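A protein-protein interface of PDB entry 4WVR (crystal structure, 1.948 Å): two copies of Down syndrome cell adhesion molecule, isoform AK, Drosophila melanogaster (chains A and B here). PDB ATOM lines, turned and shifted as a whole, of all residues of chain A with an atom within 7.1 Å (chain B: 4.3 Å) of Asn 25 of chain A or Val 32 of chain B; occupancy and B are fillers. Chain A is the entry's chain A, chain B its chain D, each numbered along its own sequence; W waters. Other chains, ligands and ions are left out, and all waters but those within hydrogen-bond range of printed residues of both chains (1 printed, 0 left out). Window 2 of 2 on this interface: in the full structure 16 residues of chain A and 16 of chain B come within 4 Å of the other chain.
The backbone NH (N) of Gly 27 of chain A is in hydrogen-bond range of the side-chain sulfur (SD) of Met 31 of chain B, at 3.4 Å.
The side-chain amide oxygen (OE1) of Gln 33 of chain B is in hydrogen-bond range of the backbone NH (N) of Asn 25 of chain A (2.8 Å).
ND2 of Asn 25 of chain A is in hydrogen-bond range of OG1 of Thr 66 of chain B.
O of Asn 25 of chain A sits close to SD of Met 31 of chain B (3.8 Å).
O of Val 32 of chain B sits at hydrogen-bond distance from ND2 of Asn 25 of chain A, at 3.2 Å.
ND2 of Asn 25 of chain A is in hydrogen-bond range of O of Lys 65 of chain B (3.3 Å).
The side-chain amide nitrogen (ND2) of Asn 70 of chain A is in hydrogen-bond range of the side-chain hydroxyl (OG1) of Thr 66 of chain B, at 3.4 Å.
The side-chain carboxylate (OE2) of Glu 24 of chain A lies within hydrogen-bond range of the backbone NH (N) of Asn 21 of chain A, 3.2 Å away.
N of Ala 72 of chain A lies within hydrogen-bond range of OD1 of Asn 70 of chain A.
O of Ala 26 of chain A lies within hydrogen-bond range of ND2 of Asn 70 of chain A (3.2 Å).
The backbone NH (N) of Gln 33 of chain B is in hydrogen-bond range of the backbone carbonyl oxygen (O) of Ser 9 of chain B, 2.7 Å away.
O of Gln 33 of chain B lies within hydrogen-bond range of NZ of Lys 65 of chain B (3.0 Å).
The backbone NH (N) of Val 32 of chain B is in hydrogen-bond range of the backbone carbonyl oxygen (O) of Lys 65 of chain B (2.7 Å).
CB of Glu 24 of chain A touches OE1 of Gln 33 of chain B, 3.4 Å away.
Ala 26 of chain A touches Met 31 of chain B.
SD of Met 31 of chain B touches ND2 of Asn 70 of chain A, at 3.8 Å.
Of chain B, only Met 31 (3.3 Å), Val 32 (3.2 Å), Gln 33 (2.8 Å), Lys 65 (3.3 Å) and Thr 66 (2.8 Å) come within 4 Å of Asn 25 of chain A.
Printed residues of chain A within 4 Å of Met 31 of chain B: Asn 25 (3.3 Å), Ala 26 (3.6 Å), Gly 27 (3.4 Å) and Asn 70 (3.8 Å).
Of chain A, only Asn 25 (3.2 Å) comes within 4 Å of Val 32 of chain B.
Of the printed residues of chain A, Gln 33 of chain B touches Glu 24 (3.4 Å) and Asn 25 (2.8 Å).
Ile 41 of chain B touches none of the printed residues of chain A.
The nearest printed residue of chain B that does not touch Asn 25 of chain A is Cys 30 of chain B (5.4 Å).
The nearest printed residue of chain A that does not touch Thr 66 of chain B is Ala 72 of chain A (6.0 Å).
Of the 11 printed residues of chain B, 5 touch a printed residue of chain A.
Among the printed residues, no Asp or Glu carboxylate lies within 4 Å of a Lys or Arg side-chain nitrogen of the other chain.
No position is printed for both chains.
Of the 10 pairs that touch across the chains among the printed residues, none has its exchanged pair printed and touching as well.
Water W1 lies within hydrogen-bond range of OG1 of Thr 66 of chain B (2.8 Å), OD1 of Asn 70 of chain A (2.8 Å) and OD1 of Asn 25 of chain A (3.3 Å).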
ATOM      1  N   VAL A  20      -6.936 -24.113   4.774  1.00  0.00           N
ATOM      2  CA  VAL A  20      -6.601 -23.077   3.813  1.00  0.00           C
ATOM      3  C   VAL A  20      -5.718 -23.653   2.709  1.00  0.00           C
ATOM      4  O   VAL A  20      -4.871 -24.505   2.970  1.00  0.00           O
ATOM      5  CB  VAL A  20      -5.890 -21.896   4.511  1.00  0.00           C
ATOM      6  CG1 VAL A  20      -5.568 -20.798   3.527  1.00  0.00           C
ATOM      7  CG2 VAL A  20      -6.758 -21.353   5.641  1.00  0.00           C
ATOM      8  N   ASN A  21      -5.927 -23.205   1.476  1.00  0.00           N
ATOM      9  CA  ASN A  21      -5.086 -23.633   0.369  1.00  0.00           C
ATOM     10  C   ASN A  21      -3.754 -22.901   0.358  1.00  0.00           C
ATOM     11  O   ASN A  21      -3.646 -21.772   0.842  1.00  0.00           O
ATOM     12  CB  ASN A  21      -5.800 -23.427  -0.967  1.00  0.00           C
ATOM     13  CG  ASN A  21      -6.863 -24.473  -1.228  1.00  0.00           C
ATOM     14  OD1 ASN A  21      -8.016 -24.147  -1.503  1.00  0.00           O
ATOM     15  ND2 ASN A  21      -6.477 -25.741  -1.136  1.00  0.00           N
ATOM     16  N   THR A  22      -2.738 -23.557  -0.194  1.00  0.00           N
ATOM     17  CA  THR A  22      -1.427 -22.946  -0.356  1.00  0.00           C
ATOM     18  C   THR A  22      -1.518 -21.711  -1.249  1.00  0.00           C
ATOM     19  O   THR A  22      -2.173 -21.737  -2.289  1.00  0.00           O
ATOM     20  CB  THR A  22      -0.414 -23.944  -0.954  1.00  0.00           C
ATOM     21  OG1 THR A  22      -0.219 -25.030  -0.041  1.00  0.00           O
ATOM     22  CG2 THR A  22       0.921 -23.269  -1.210  1.00  0.00           C
ATOM     23  N   GLY A  23      -0.877 -20.628  -0.825  1.00  0.00           N
ATOM     24  CA  GLY A  23      -0.855 -19.404  -1.603  1.00  0.00           C
ATOM     25  C   GLY A  23      -1.855 -18.363  -1.141  1.00  0.00           C
ATOM     26  O   GLY A  23      -1.813 -17.216  -1.586  1.00  0.00           O
ATOM     27  N   GLU A  24      -2.760 -18.751  -0.250  1.00  0.00           N
ATOM     28  CA  GLU A  24      -3.771 -17.818   0.236  1.00  0.00           C
ATOM     29  C   GLU A  24      -3.187 -16.796   1.207  1.00  0.00           C
ATOM     30  O   GLU A  24      -2.083 -16.964   1.727  1.00  0.00           O
ATOM     31  CB  GLU A  24      -4.926 -18.557   0.909  1.00  0.00           C
ATOM     32  CG  GLU A  24      -5.794 -19.377  -0.040  1.00  0.00           C
ATOM     33  CD  GLU A  24      -7.096 -19.823   0.605  1.00  0.00           C
ATOM     34  OE1 GLU A  24      -7.580 -19.124   1.522  1.00  0.00           O
ATOM     35  OE2 GLU A  24      -7.634 -20.876   0.200  1.00  0.00           O
ATOM     36  N   ASN A  25      -3.952 -15.736   1.439  1.00  0.00           N
ATOM     37  CA  ASN A  25      -3.565 -14.643   2.320  1.00  0.00           C
ATOM     38  C   ASN A  25      -4.359 -14.744   3.615  1.00  0.00           C
ATOM     39  O   ASN A  25      -5.560 -14.481   3.633  1.00  0.00           O
ATOM     40  CB  ASN A  25      -3.807 -13.306   1.613  1.00  0.00           C
ATOM     41  CG  ASN A  25      -3.553 -12.099   2.501  1.00  0.00           C
ATOM     42  OD1 ASN A  25      -2.903 -12.190   3.542  1.00  0.00           O
ATOM     43  ND2 ASN A  25      -4.065 -10.951   2.077  1.00  0.00           N
ATOM     44  N   ALA A  26      -3.692 -15.146   4.692  1.00  0.00           N
ATOM     45  CA  ALA A  26      -4.374 -15.384   5.957  1.00  0.00           C
ATOM     46  C   ALA A  26      -3.804 -14.507   7.057  1.00  0.00           C
ATOM     47  O   ALA A  26      -2.654 -14.066   6.987  1.00  0.00           O
ATOM     48  CB  ALA A  26      -4.279 -16.851   6.347  1.00  0.00           C
ATOM     49  N   GLY A  27      -4.614 -14.250   8.076  1.00  0.00           N
ATOM     50  CA  GLY A  27      -4.173 -13.406   9.168  1.00  0.00           C
ATOM     51  C   GLY A  27      -5.161 -13.308  10.309  1.00  0.00           C
ATOM     52  O   GLY A  27      -6.325 -13.689  10.172  1.00  0.00           O
ATOM     53  N   ASN A  70       0.046 -11.513   9.806  1.00  0.00           N
ATOM     54  CA  ASN A  70      -0.349 -11.777   8.426  1.00  0.00           C
ATOM     55  C   ASN A  70       0.582 -12.776   7.758  1.00  0.00           C
ATOM     56  O   ASN A  70       1.802 -12.690   7.888  1.00  0.00           O
ATOM     57  CB  ASN A  70      -0.385 -10.477   7.608  1.00  0.00           C
ATOM     58  CG  ASN A  70      -0.866 -10.697   6.181  1.00  0.00           C
ATOM     59  OD1 ASN A  70      -0.096 -10.588   5.224  1.00  0.00           O
ATOM     60  ND2 ASN A  70      -2.146 -11.020   6.033  1.00  0.00           N
ATOM     61  N   ILE A  71      -0.005 -13.730   7.049  1.00  0.00           N
ATOM     62  CA  ILE A  71       0.767 -14.644   6.226  1.00  0.00           C
ATOM     63  C   ILE A  71       0.410 -14.368   4.776  1.00  0.00           C
ATOM     64  O   ILE A  71      -0.626 -14.823   4.289  1.00  0.00           O
ATOM     65  CB  ILE A  71       0.492 -16.113   6.578  1.00  0.00           C
ATOM     66  CG1 ILE A  71       0.688 -16.341   8.079  1.00  0.00           C
ATOM     67  CG2 ILE A  71       1.392 -17.032   5.757  1.00  0.00           C
ATOM     68  CD1 ILE A  71       0.352 -17.751   8.531  1.00  0.00           C
ATOM     69  N   ALA A  72       1.263 -13.599   4.104  1.00  0.00           N
ATOM     70  CA  ALA A  72       0.970 -13.096   2.763  1.00  0.00           C
ATOM     71  C   ALA A  72       0.712 -14.212   1.751  1.00  0.00           C
ATOM     72  O   ALA A  72      -0.175 -14.098   0.904  1.00  0.00           O
ATOM     73  CB  ALA A  72       2.108 -12.205   2.286  1.00  0.00           C
ATOM     74  N   ALA A  73       1.498 -15.282   1.844  1.00  0.00           N
ATOM     75  CA  ALA A  73       1.333 -16.448   0.980  1.00  0.00           C
ATOM     76  C   ALA A  73       1.493 -17.721   1.801  1.00  0.00           C
ATOM     77  O   ALA A  73       2.611 -18.133   2.109  1.00  0.00           O
ATOM     78  CB  ALA A  73       2.334 -16.420  -0.163  1.00  0.00           C
ATOM     79  N   VAL A  74       0.370 -18.336   2.154  1.00  0.00           N
ATOM     80  CA  VAL A  74       0.379 -19.517   3.009  1.00  0.00           C
ATOM     81  C   VAL A  74       1.028 -20.719   2.327  1.00  0.00           C
ATOM     82  O   VAL A  74       0.674 -21.073   1.205  1.00  0.00           O
ATOM     83  CB  VAL A  74      -1.048 -19.906   3.443  1.00  0.00           C
ATOM     84  CG1 VAL A  74      -1.045 -21.257   4.148  1.00  0.00           C
ATOM     85  CG2 VAL A  74      -1.649 -18.825   4.341  1.00  0.00           C
ATOM     86  N   SER B   9     -10.170 -10.813  -5.341  1.00  0.00           N
ATOM     87  CA  SER B   9     -11.118 -11.533  -4.500  1.00  0.00           C
ATOM     88  C   SER B   9     -10.754 -11.274  -3.043  1.00  0.00           C
ATOM     89  O   SER B   9      -9.577 -11.135  -2.716  1.00  0.00           O
ATOM     90  CB  SER B   9     -11.104 -13.028  -4.807  1.00  0.00           C
ATOM     91  OG  SER B   9      -9.918 -13.645  -4.344  1.00  0.00           O
ATOM     92  N   CYS B  30      -9.064  -6.658   5.726  1.00  0.00           N
ATOM     93  CA  CYS B  30      -9.444  -6.864   4.338  1.00  0.00           C
ATOM     94  C   CYS B  30      -8.290  -7.526   3.608  1.00  0.00           C
ATOM     95  O   CYS B  30      -7.333  -6.865   3.209  1.00  0.00           O
ATOM     96  CB  CYS B  30      -9.825  -5.551   3.660  1.00  0.00           C
ATOM     97  SG  CYS B  30     -10.449  -5.800   1.981  1.00  0.00           S
ATOM     98  N   MET B  31      -8.378  -8.842   3.451  1.00  0.00           N
ATOM     99  CA  MET B  31      -7.285  -9.604   2.875  1.00  0.00           C
ATOM    100  C   MET B  31      -7.638 -10.071   1.473  1.00  0.00           C
ATOM    101  O   MET B  31      -8.488 -10.952   1.283  1.00  0.00           O
ATOM    102  CB  MET B  31      -6.929 -10.790   3.777  1.00  0.00           C
ATOM    103  CG  MET B  31      -6.258 -10.374   5.088  1.00  0.00           C
ATOM    104  SD  MET B  31      -5.898 -11.730   6.230  1.00  0.00           S
ATOM    105  CE  MET B  31      -7.553 -12.138   6.782  1.00  0.00           C
ATOM    106  N   VAL B  32      -6.988  -9.456   0.493  1.00  0.00           N
ATOM    107  CA  VAL B  32      -7.177  -9.814  -0.902  1.00  0.00           C
ATOM    108  C   VAL B  32      -6.482 -11.139  -1.171  1.00  0.00           C
ATOM    109  O   VAL B  32      -5.327 -11.332  -0.790  1.00  0.00           O
ATOM    110  CB  VAL B  32      -6.630  -8.727  -1.841  1.00  0.00           C
ATOM    111  CG1 VAL B  32      -6.722  -9.176  -3.297  1.00  0.00           C
ATOM    112  CG2 VAL B  32      -7.386  -7.420  -1.621  1.00  0.00           C
ATOM    113  N   GLN B  33      -7.197 -12.061  -1.806  1.00  0.00           N
ATOM    114  CA  GLN B  33      -6.652 -13.384  -2.065  1.00  0.00           C
ATOM    115  C   GLN B  33      -5.997 -13.416  -3.436  1.00  0.00           C
ATOM    116  O   GLN B  33      -4.796 -13.191  -3.556  1.00  0.00           O
ATOM    117  CB  GLN B  33      -7.748 -14.441  -1.944  1.00  0.00           C
ATOM    118  CG  GLN B  33      -8.378 -14.466  -0.558  1.00  0.00           C
ATOM    119  CD  GLN B  33      -7.344 -14.687   0.528  1.00  0.00           C
ATOM    120  OE1 GLN B  33      -6.544 -15.621   0.454  1.00  0.00           O
ATOM    121  NE2 GLN B  33      -7.345 -13.820   1.542  1.00  0.00           N
ATOM    122  N   LYS B  34      -6.778 -13.686  -4.473  1.00  0.00           N
ATOM    123  CA  LYS B  34      -6.244 -13.610  -5.825  1.00  0.00           C
ATOM    124  C   LYS B  34      -6.366 -12.174  -6.329  1.00  0.00           C
ATOM    125  O   LYS B  34      -7.143 -11.383  -5.790  1.00  0.00           O
ATOM    126  CB  LYS B  34      -6.968 -14.588  -6.756  1.00  0.00           C
ATOM    127  CG  LYS B  34      -6.808 -16.051  -6.354  1.00  0.00           C
ATOM    128  CD  LYS B  34      -6.839 -16.972  -7.561  1.00  0.00           C
ATOM    129  CE  LYS B  34      -6.043 -18.248  -7.309  1.00  0.00           C
ATOM    130  NZ  LYS B  34      -4.731 -18.248  -8.027  1.00  0.00           N
ATOM    131  N   ILE B  39      -3.015  -3.063  -6.862  1.00  0.00           N
ATOM    132  CA  ILE B  39      -4.369  -3.094  -6.327  1.00  0.00           C
ATOM    133  C   ILE B  39      -4.570  -1.904  -5.410  1.00  0.00           C
ATOM    134  O   ILE B  39      -3.660  -1.531  -4.670  1.00  0.00           O
ATOM    135  CB  ILE B  39      -4.649  -4.384  -5.521  1.00  0.00           C
ATOM    136  CG1 ILE B  39      -4.401  -5.618  -6.372  1.00  0.00           C
ATOM    137  CG2 ILE B  39      -6.082  -4.405  -4.995  1.00  0.00           C
ATOM    138  CD1 ILE B  39      -4.836  -6.910  -5.707  1.00  0.00           C
ATOM    139  N   ILE B  41      -6.983  -0.585  -2.237  1.00  0.00           N
ATOM    140  CA  ILE B  41      -7.926  -1.009  -1.211  1.00  0.00           C
ATOM    141  C   ILE B  41      -8.440   0.220  -0.477  1.00  0.00           C
ATOM    142  O   ILE B  41      -7.656   1.077  -0.080  1.00  0.00           O
ATOM    143  CB  ILE B  41      -7.280  -1.992  -0.209  1.00  0.00           C
ATOM    144  CG1 ILE B  41      -6.767  -3.237  -0.938  1.00  0.00           C
ATOM    145  CG2 ILE B  41      -8.269  -2.379   0.881  1.00  0.00           C
ATOM    146  CD1 ILE B  41      -6.105  -4.264  -0.022  1.00  0.00           C
ATOM    147  N   LYS B  65      -1.787  -6.354  -0.416  1.00  0.00           N
ATOM    148  CA  LYS B  65      -3.029  -7.118  -0.477  1.00  0.00           C
ATOM    149  C   LYS B  65      -3.787  -7.203   0.847  1.00  0.00           C
ATOM    150  O   LYS B  65      -4.794  -7.912   0.945  1.00  0.00           O
ATOM    151  CB  LYS B  65      -2.744  -8.531  -0.991  1.00  0.00           C
ATOM    152  CG  LYS B  65      -2.416  -8.580  -2.476  1.00  0.00           C
ATOM    153  CD  LYS B  65      -2.608  -9.979  -3.022  1.00  0.00           C
ATOM    154  CE  LYS B  65      -2.599  -9.989  -4.536  1.00  0.00           C
ATOM    155  NZ  LYS B  65      -2.977 -11.330  -5.067  1.00  0.00           N
ATOM    156  N   THR B  66      -3.327  -6.477   1.860  1.00  0.00           N
ATOM    157  CA  THR B  66      -3.975  -6.533   3.169  1.00  0.00           C
ATOM    158  C   THR B  66      -4.151  -5.155   3.807  1.00  0.00           C
ATOM    159  O   THR B  66      -3.185  -4.406   3.996  1.00  0.00           O
ATOM    160  CB  THR B  66      -3.188  -7.427   4.152  1.00  0.00           C
ATOM    161  OG1 THR B  66      -3.134  -8.771   3.651  1.00  0.00           O
ATOM    162  CG2 THR B  66      -3.851  -7.422   5.519  1.00  0.00           C
ATOM    163  N   ALA B  86     -11.789  -3.451  -3.151  1.00  0.00           N
ATOM    164  CA  ALA B  86     -10.501  -3.752  -3.765  1.00  0.00           C
ATOM    165  C   ALA B  86     -10.609  -3.675  -5.286  1.00  0.00           C
ATOM    166  O   ALA B  86     -11.478  -4.309  -5.885  1.00  0.00           O
ATOM    167  CB  ALA B  86     -10.013  -5.120  -3.329  1.00  0.00           C
HETATM  168  O   HOH W   1      -0.799  -9.832   2.638  1.00  0.00           O
